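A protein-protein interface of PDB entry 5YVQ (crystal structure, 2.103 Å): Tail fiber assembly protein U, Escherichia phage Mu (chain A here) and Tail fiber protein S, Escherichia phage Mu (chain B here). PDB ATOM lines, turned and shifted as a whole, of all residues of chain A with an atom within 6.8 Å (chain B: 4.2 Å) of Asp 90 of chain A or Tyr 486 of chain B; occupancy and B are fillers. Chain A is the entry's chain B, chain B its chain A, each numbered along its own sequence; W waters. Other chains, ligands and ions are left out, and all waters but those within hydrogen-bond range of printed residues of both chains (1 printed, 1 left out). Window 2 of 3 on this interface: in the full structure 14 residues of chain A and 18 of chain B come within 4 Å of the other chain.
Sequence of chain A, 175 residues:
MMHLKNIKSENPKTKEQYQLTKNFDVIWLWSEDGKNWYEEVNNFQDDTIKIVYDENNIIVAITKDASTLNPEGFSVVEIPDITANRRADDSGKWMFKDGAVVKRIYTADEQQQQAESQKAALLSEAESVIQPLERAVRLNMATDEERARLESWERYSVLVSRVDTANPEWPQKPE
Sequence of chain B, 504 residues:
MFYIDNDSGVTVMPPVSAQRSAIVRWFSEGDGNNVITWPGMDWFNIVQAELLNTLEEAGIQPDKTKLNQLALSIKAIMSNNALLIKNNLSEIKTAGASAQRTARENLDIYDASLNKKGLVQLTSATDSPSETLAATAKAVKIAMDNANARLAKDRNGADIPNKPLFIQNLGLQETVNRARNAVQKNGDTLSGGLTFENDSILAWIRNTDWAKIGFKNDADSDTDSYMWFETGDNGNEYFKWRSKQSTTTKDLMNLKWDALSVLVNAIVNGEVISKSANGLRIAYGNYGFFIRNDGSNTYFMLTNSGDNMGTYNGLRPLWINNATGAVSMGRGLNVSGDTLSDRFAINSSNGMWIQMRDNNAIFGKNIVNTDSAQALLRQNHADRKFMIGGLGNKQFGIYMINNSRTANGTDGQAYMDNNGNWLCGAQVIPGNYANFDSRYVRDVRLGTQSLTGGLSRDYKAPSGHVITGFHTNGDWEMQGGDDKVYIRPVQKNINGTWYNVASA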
ATOM      1  N   ILE A  58      -3.981  -9.880 -25.295  1.00  0.00           N
ATOM      2  CA  ILE A  58      -5.332 -10.072 -24.774  1.00  0.00           C
ATOM      3  C   ILE A  58      -6.312  -9.474 -25.776  1.00  0.00           C
ATOM      4  O   ILE A  58      -6.148  -8.328 -26.210  1.00  0.00           O
ATOM      5  CB  ILE A  58      -5.501  -9.419 -23.387  1.00  0.00           C
ATOM      6  CG1 ILE A  58      -4.810 -10.213 -22.271  1.00  0.00           C
ATOM      7  CG2 ILE A  58      -6.976  -9.264 -23.040  1.00  0.00           C
ATOM      8  CD1 ILE A  58      -3.314 -10.349 -22.377  1.00  0.00           C
ATOM      9  N   ILE A  59      -7.328 -10.241 -26.156  1.00  0.00           N
ATOM     10  CA  ILE A  59      -8.318  -9.753 -27.110  1.00  0.00           C
ATOM     11  C   ILE A  59      -9.262  -8.800 -26.388  1.00  0.00           C
ATOM     12  O   ILE A  59      -9.922  -9.180 -25.414  1.00  0.00           O
ATOM     13  CB  ILE A  59      -9.086 -10.910 -27.761  1.00  0.00           C
ATOM     14  CG1 ILE A  59      -8.134 -11.805 -28.554  1.00  0.00           C
ATOM     15  CG2 ILE A  59     -10.181 -10.374 -28.674  1.00  0.00           C
ATOM     16  CD1 ILE A  59      -8.593 -13.235 -28.638  1.00  0.00           C
ATOM     17  N   VAL A  60      -9.320  -7.557 -26.861  1.00  0.00           N
ATOM     18  CA  VAL A  60     -10.165  -6.541 -26.250  1.00  0.00           C
ATOM     19  C   VAL A  60     -11.380  -6.182 -27.102  1.00  0.00           C
ATOM     20  O   VAL A  60     -12.354  -5.637 -26.558  1.00  0.00           O
ATOM     21  CB  VAL A  60      -9.356  -5.267 -25.922  1.00  0.00           C
ATOM     22  CG1 VAL A  60      -8.206  -5.590 -24.989  1.00  0.00           C
ATOM     23  CG2 VAL A  60      -8.854  -4.604 -27.208  1.00  0.00           C
ATOM     24  N   ALA A  61     -11.364  -6.464 -28.404  1.00  0.00           N
ATOM     25  CA  ALA A  61     -12.476  -6.095 -29.267  1.00  0.00           C
ATOM     26  C   ALA A  61     -12.593  -7.095 -30.408  1.00  0.00           C
ATOM     27  O   ALA A  61     -11.582  -7.559 -30.943  1.00  0.00           O
ATOM     28  CB  ALA A  61     -12.310  -4.677 -29.820  1.00  0.00           C
ATOM     29  N   ILE A  62     -13.833  -7.420 -30.770  1.00  0.00           N
ATOM     30  CA  ILE A  62     -14.127  -8.344 -31.858  1.00  0.00           C
ATOM     31  C   ILE A  62     -15.243  -7.749 -32.705  1.00  0.00           C
ATOM     32  O   ILE A  62     -16.171  -7.124 -32.179  1.00  0.00           O
ATOM     33  CB  ILE A  62     -14.522  -9.742 -31.333  1.00  0.00           C
ATOM     34  CG1 ILE A  62     -13.414 -10.321 -30.451  1.00  0.00           C
ATOM     35  CG2 ILE A  62     -14.811 -10.696 -32.483  1.00  0.00           C
ATOM     36  CD1 ILE A  62     -13.920 -11.248 -29.379  1.00  0.00           C
ATOM     37  N   ALA A  88     -15.004 -16.741 -28.548  1.00  0.00           N
ATOM     38  CA  ALA A  88     -14.246 -15.655 -27.939  1.00  0.00           C
ATOM     39  C   ALA A  88     -15.102 -14.399 -27.843  1.00  0.00           C
ATOM     40  O   ALA A  88     -15.712 -13.975 -28.829  1.00  0.00           O
ATOM     41  CB  ALA A  88     -12.980 -15.372 -28.746  1.00  0.00           C
ATOM     42  N   ASP A  89     -15.150 -13.807 -26.653  1.00  0.00           N
ATOM     43  CA  ASP A  89     -15.858 -12.556 -26.419  1.00  0.00           C
ATOM     44  C   ASP A  89     -14.858 -11.431 -26.176  1.00  0.00           C
ATOM     45  O   ASP A  89     -13.649 -11.651 -26.063  1.00  0.00           O
ATOM     46  CB  ASP A  89     -16.832 -12.684 -25.238  1.00  0.00           C
ATOM     47  CG  ASP A  89     -16.222 -13.397 -24.040  1.00  0.00           C
ATOM     48  OD1 ASP A  89     -14.979 -13.467 -23.940  1.00  0.00           O
ATOM     49  OD2 ASP A  89     -16.996 -13.890 -23.193  1.00  0.00           O
ATOM     50  N   ASP A  90     -15.382 -10.207 -26.109  1.00  0.00           N
ATOM     51  CA  ASP A  90     -14.538  -9.028 -25.947  1.00  0.00           C
ATOM     52  C   ASP A  90     -13.909  -8.923 -24.563  1.00  0.00           C
ATOM     53  O   ASP A  90     -13.125  -7.994 -24.334  1.00  0.00           O
ATOM     54  CB  ASP A  90     -15.341  -7.760 -26.244  1.00  0.00           C
ATOM     55  CG  ASP A  90     -16.588  -7.644 -25.389  1.00  0.00           C
ATOM     56  OD1 ASP A  90     -17.144  -8.689 -24.993  1.00  0.00           O
ATOM     57  OD2 ASP A  90     -17.011  -6.502 -25.113  1.00  0.00           O
ATOM     58  N   SER A  91     -14.225  -9.829 -23.642  1.00  0.00           N
ATOM     59  CA  SER A  91     -13.597  -9.810 -22.332  1.00  0.00           C
ATOM     60  C   SER A  91     -12.148 -10.289 -22.427  1.00  0.00           C
ATOM     61  O   SER A  91     -11.677 -10.749 -23.472  1.00  0.00           O
ATOM     62  CB  SER A  91     -14.376 -10.677 -21.347  1.00  0.00           C
ATOM     63  OG  SER A  91     -13.719 -10.709 -20.096  1.00  0.00           O
ATOM     64  N   GLY A  92     -11.440 -10.185 -21.307  1.00  0.00           N
ATOM     65  CA  GLY A  92     -10.034 -10.529 -21.290  1.00  0.00           C
ATOM     66  C   GLY A  92      -9.775 -11.998 -21.034  1.00  0.00           C
ATOM     67  O   GLY A  92      -8.708 -12.360 -20.527  1.00  0.00           O
ATOM     68  N   LYS A  93     -10.733 -12.856 -21.382  1.00  0.00           N
ATOM     69  CA  LYS A  93     -10.625 -14.287 -21.139  1.00  0.00           C
ATOM     70  C   LYS A  93     -10.114 -15.058 -22.349  1.00  0.00           C
ATOM     71  O   LYS A  93     -10.082 -16.292 -22.315  1.00  0.00           O
ATOM     72  CB  LYS A  93     -11.978 -14.850 -20.693  1.00  0.00           C
ATOM     73  CG  LYS A  93     -12.223 -14.739 -19.193  1.00  0.00           C
ATOM     74  CD  LYS A  93     -13.706 -14.638 -18.870  1.00  0.00           C
ATOM     75  CE  LYS A  93     -14.454 -15.881 -19.321  1.00  0.00           C
ATOM     76  NZ  LYS A  93     -15.487 -16.291 -18.328  1.00  0.00           N
ATOM     77  N   TRP A  94      -9.718 -14.365 -23.415  1.00  0.00           N
ATOM     78  CA  TRP A  94      -9.196 -15.011 -24.610  1.00  0.00           C
ATOM     79  C   TRP A  94      -7.998 -14.227 -25.122  1.00  0.00           C
ATOM     80  O   TRP A  94      -8.010 -12.994 -25.125  1.00  0.00           O
ATOM     81  CB  TRP A  94     -10.260 -15.114 -25.712  1.00  0.00           C
ATOM     82  CG  TRP A  94     -11.557 -15.706 -25.254  1.00  0.00           C
ATOM     83  CD1 TRP A  94     -12.543 -15.075 -24.554  1.00  0.00           C
ATOM     84  CD2 TRP A  94     -12.016 -17.046 -25.471  1.00  0.00           C
ATOM     85  NE1 TRP A  94     -13.585 -15.938 -24.317  1.00  0.00           N
ATOM     86  CE2 TRP A  94     -13.286 -17.155 -24.869  1.00  0.00           C
ATOM     87  CE3 TRP A  94     -11.472 -18.166 -26.111  1.00  0.00           C
ATOM     88  CZ2 TRP A  94     -14.023 -18.339 -24.889  1.00  0.00           C
ATOM     89  CZ3 TRP A  94     -12.206 -19.341 -26.130  1.00  0.00           C
ATOM     90  CH2 TRP A  94     -13.468 -19.418 -25.523  1.00  0.00           C
ATOM     91  N   GLN B 449     -17.596  -2.030 -29.615  1.00  0.00           N
ATOM     92  CA  GLN B 449     -17.321  -1.964 -28.186  1.00  0.00           C
ATOM     93  C   GLN B 449     -16.065  -2.762 -27.835  1.00  0.00           C
ATOM     94  O   GLN B 449     -15.873  -3.887 -28.308  1.00  0.00           O
ATOM     95  CB  GLN B 449     -18.530  -2.501 -27.424  1.00  0.00           C
ATOM     96  CG  GLN B 449     -18.554  -2.196 -25.946  1.00  0.00           C
ATOM     97  CD  GLN B 449     -19.869  -2.600 -25.309  1.00  0.00           C
ATOM     98  OE1 GLN B 449     -20.487  -1.815 -24.593  1.00  0.00           O
ATOM     99  NE2 GLN B 449     -20.300  -3.834 -25.562  1.00  0.00           N
ATOM    100  N   SER B 450     -15.203  -2.174 -27.010  1.00  0.00           N
ATOM    101  CA  SER B 450     -14.026  -2.856 -26.492  1.00  0.00           C
ATOM    102  C   SER B 450     -13.989  -2.709 -24.975  1.00  0.00           C
ATOM    103  O   SER B 450     -14.708  -1.892 -24.392  1.00  0.00           O
ATOM    104  CB  SER B 450     -12.727  -2.309 -27.109  1.00  0.00           C
ATOM    105  OG  SER B 450     -12.259  -1.168 -26.411  1.00  0.00           O
ATOM    106  N   LEU B 451     -13.143  -3.512 -24.334  1.00  0.00           N
ATOM    107  CA  LEU B 451     -12.956  -3.441 -22.891  1.00  0.00           C
ATOM    108  C   LEU B 451     -11.525  -3.082 -22.543  1.00  0.00           C
ATOM    109  O   LEU B 451     -10.577  -3.632 -23.109  1.00  0.00           O
ATOM    110  CB  LEU B 451     -13.308  -4.749 -22.195  1.00  0.00           C
ATOM    111  CG  LEU B 451     -14.718  -4.603 -21.645  1.00  0.00           C
ATOM    112  CD1 LEU B 451     -15.634  -4.853 -22.809  1.00  0.00           C
ATOM    113  CD2 LEU B 451     -15.025  -5.517 -20.459  1.00  0.00           C
ATOM    114  N   ILE B 467     -17.455   6.177 -22.776  1.00  0.00           N
ATOM    115  CA  ILE B 467     -17.747   5.023 -21.928  1.00  0.00           C
ATOM    116  C   ILE B 467     -19.161   4.530 -22.202  1.00  0.00           C
ATOM    117  O   ILE B 467     -20.128   5.303 -22.168  1.00  0.00           O
ATOM    118  CB  ILE B 467     -17.560   5.367 -20.444  1.00  0.00           C
ATOM    119  CG1 ILE B 467     -16.084   5.282 -20.080  1.00  0.00           C
ATOM    120  CG2 ILE B 467     -18.353   4.404 -19.560  1.00  0.00           C
ATOM    121  CD1 ILE B 467     -15.673   6.316 -19.123  1.00  0.00           C
ATOM    122  N   THR B 468     -19.285   3.224 -22.448  1.00  0.00           N
ATOM    123  CA  THR B 468     -20.559   2.602 -22.771  1.00  0.00           C
ATOM    124  C   THR B 468     -20.916   1.431 -21.855  1.00  0.00           C
ATOM    125  O   THR B 468     -21.912   0.747 -22.113  1.00  0.00           O
ATOM    126  CB  THR B 468     -20.555   2.125 -24.230  1.00  0.00           C
ATOM    127  OG1 THR B 468     -19.344   1.397 -24.478  1.00  0.00           O
ATOM    128  CG2 THR B 468     -20.639   3.318 -25.202  1.00  0.00           C
ATOM    129  N   GLY B 469     -20.149   1.169 -20.803  1.00  0.00           N
ATOM    130  CA  GLY B 469     -20.539   0.107 -19.891  1.00  0.00           C
ATOM    131  C   GLY B 469     -19.531  -0.102 -18.780  1.00  0.00           C
ATOM    132  O   GLY B 469     -18.581   0.664 -18.619  1.00  0.00           O
ATOM    133  N   PHE B 470     -19.762  -1.164 -18.006  1.00  0.00           N
ATOM    134  CA  PHE B 470     -18.916  -1.495 -16.865  1.00  0.00           C
ATOM    135  C   PHE B 470     -18.841  -3.004 -16.699  1.00  0.00           C
ATOM    136  O   PHE B 470     -19.726  -3.744 -17.137  1.00  0.00           O
ATOM    137  CB  PHE B 470     -19.432  -0.875 -15.562  1.00  0.00           C
ATOM    138  CG  PHE B 470     -19.803   0.571 -15.678  1.00  0.00           C
ATOM    139  CD1 PHE B 470     -21.125   0.947 -15.850  1.00  0.00           C
ATOM    140  CD2 PHE B 470     -18.833   1.558 -15.611  1.00  0.00           C
ATOM    141  CE1 PHE B 470     -21.471   2.281 -15.961  1.00  0.00           C
ATOM    142  CE2 PHE B 470     -19.174   2.893 -15.720  1.00  0.00           C
ATOM    143  CZ  PHE B 470     -20.494   3.254 -15.893  1.00  0.00           C
ATOM    144  N   HIS B 471     -17.766  -3.451 -16.052  1.00  0.00           N
ATOM    145  CA  HIS B 471     -17.626  -4.849 -15.652  1.00  0.00           C
ATOM    146  C   HIS B 471     -16.806  -4.885 -14.369  1.00  0.00           C
ATOM    147  O   HIS B 471     -15.606  -4.600 -14.392  1.00  0.00           O
ATOM    148  CB  HIS B 471     -16.972  -5.689 -16.745  1.00  0.00           C
ATOM    149  CG  HIS B 471     -16.775  -7.123 -16.362  1.00  0.00           C
ATOM    150  ND1 HIS B 471     -17.740  -8.087 -16.563  1.00  0.00           N
ATOM    151  CD2 HIS B 471     -15.728  -7.757 -15.782  1.00  0.00           C
ATOM    152  CE1 HIS B 471     -17.294  -9.252 -16.129  1.00  0.00           C
ATOM    153  NE2 HIS B 471     -16.076  -9.079 -15.649  1.00  0.00           N
ATOM    154  N   VAL B 485     -14.190  -1.367 -17.723  1.00  0.00           N
ATOM    155  CA  VAL B 485     -15.132  -0.414 -18.300  1.00  0.00           C
ATOM    156  C   VAL B 485     -15.221  -0.659 -19.801  1.00  0.00           C
ATOM    157  O   VAL B 485     -14.211  -0.926 -20.462  1.00  0.00           O
ATOM    158  CB  VAL B 485     -14.734   1.046 -17.979  1.00  0.00           C
ATOM    159  CG1 VAL B 485     -13.366   1.387 -18.539  1.00  0.00           C
ATOM    160  CG2 VAL B 485     -15.770   2.013 -18.493  1.00  0.00           C
ATOM    161  N   TYR B 486     -16.443  -0.602 -20.328  1.00  0.00           N
ATOM    162  CA  TYR B 486     -16.694  -0.713 -21.759  1.00  0.00           C
ATOM    163  C   TYR B 486     -16.533   0.655 -22.409  1.00  0.00           C
ATOM    164  O   TYR B 486     -16.870   1.678 -21.802  1.00  0.00           O
ATOM    165  CB  TYR B 486     -18.108  -1.237 -22.021  1.00  0.00           C
ATOM    166  CG  TYR B 486     -18.351  -2.677 -21.626  1.00  0.00           C
ATOM    167  CD1 TYR B 486     -18.775  -3.602 -22.565  1.00  0.00           C
ATOM    168  CD2 TYR B 486     -18.178  -3.109 -20.313  1.00  0.00           C
ATOM    169  CE1 TYR B 486     -18.995  -4.917 -22.227  1.00  0.00           C
ATOM    170  CE2 TYR B 486     -18.403  -4.425 -19.963  1.00  0.00           C
ATOM    171  CZ  TYR B 486     -18.812  -5.323 -20.925  1.00  0.00           C
ATOM    172  OH  TYR B 486     -19.040  -6.638 -20.591  1.00  0.00           O
ATOM    173  N   ILE B 487     -16.025   0.673 -23.648  1.00  0.00           N
ATOM    174  CA  ILE B 487     -15.896   1.907 -24.416  1.00  0.00           C
ATOM    175  C   ILE B 487     -16.232   1.638 -25.880  1.00  0.00           C
ATOM    176  O   ILE B 487     -16.100   0.513 -26.373  1.00  0.00           O
ATOM    177  CB  ILE B 487     -14.485   2.543 -24.318  1.00  0.00           C
ATOM    178  CG1 ILE B 487     -13.412   1.566 -24.803  1.00  0.00           C
ATOM    179  CG2 ILE B 487     -14.192   3.049 -22.906  1.00  0.00           C
ATOM    180  CD1 ILE B 487     -12.061   2.223 -25.043  1.00  0.00           C
HETATM  181  O   HOH W   1     -15.915  -6.211 -29.021  1.00  0.00           O
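O of Val 60 of chain A lies within hydrogen-bond range of N of Leu 451 of chain B (3.2 Å).
The backbone NH (N) of Thr 468 of chain B lies within hydrogen-bond range of the backbone carbonyl oxygen (O) of Tyr 486 of chain B (2.9 Å). OE1 of Gln 449 of chain B is in hydrogen-bond range of OG1 of Thr 468 of chain B. N of Ser 450 of chain B is in hydrogen-bond range of O of Ile 487 of chain B (2.9 Å). O of Gly 469 of chain B is in hydrogen-bond range of N of Tyr 486 of chain B, at 3.0 Å.
Among the printed residues, pairs that only touch across the chains: Val 60 of chain A with Ser 450 of chain B (3.2 Å), Ala 61 of chain A with Gln 449 of chain B (3.95 Å), Ala 61 of chain A with Ser 450 of chain B (3.6 Å), Asp 90 of chain A with Leu 451 of chain B (3.2 Å) and Asp 90 of chain A with Tyr 486 of chain B (3.8 Å).
Asp 90 of chain A touches two residues of chain B. Of chain A, only Asp 90 (3.8 Å) comes within 4 Å of Tyr 486 of chain B. Printed residues of chain A within 4 Å of Leu 451 of chain B: Val 60 (3.2 Å) and Asp 90 (3.2 Å). Of the printed residues of chain B, Val 60 of chain A touches Ser 450 (3.2 Å) and Leu 451 (3.2 Å). Ile 467 of chain B touches none of the printed residues of chain A. The nearest printed residue of chain B that does not touch Asp 90 of chain A is Gln 449 of chain B (4.3 Å). The nearest residue of chain A that does not touch Tyr 486 of chain B is Ser 91 of chain A (6.2 Å).
Hydrophobic or aromatic side chains of chain A within 4 Å of the printed part of chain B: Val 60 and Ala 61. Among the printed residues, 6 pairs touch across the chains. Among the printed residues, no Asp or Glu carboxylate lies within 4 Å of a Lys or Arg side-chain nitrogen of the other chain.
Water W1 bridges the backbone carbonyl oxygen of Gln 449 of chain B and the backbone NH of Ile 62 of chain A.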
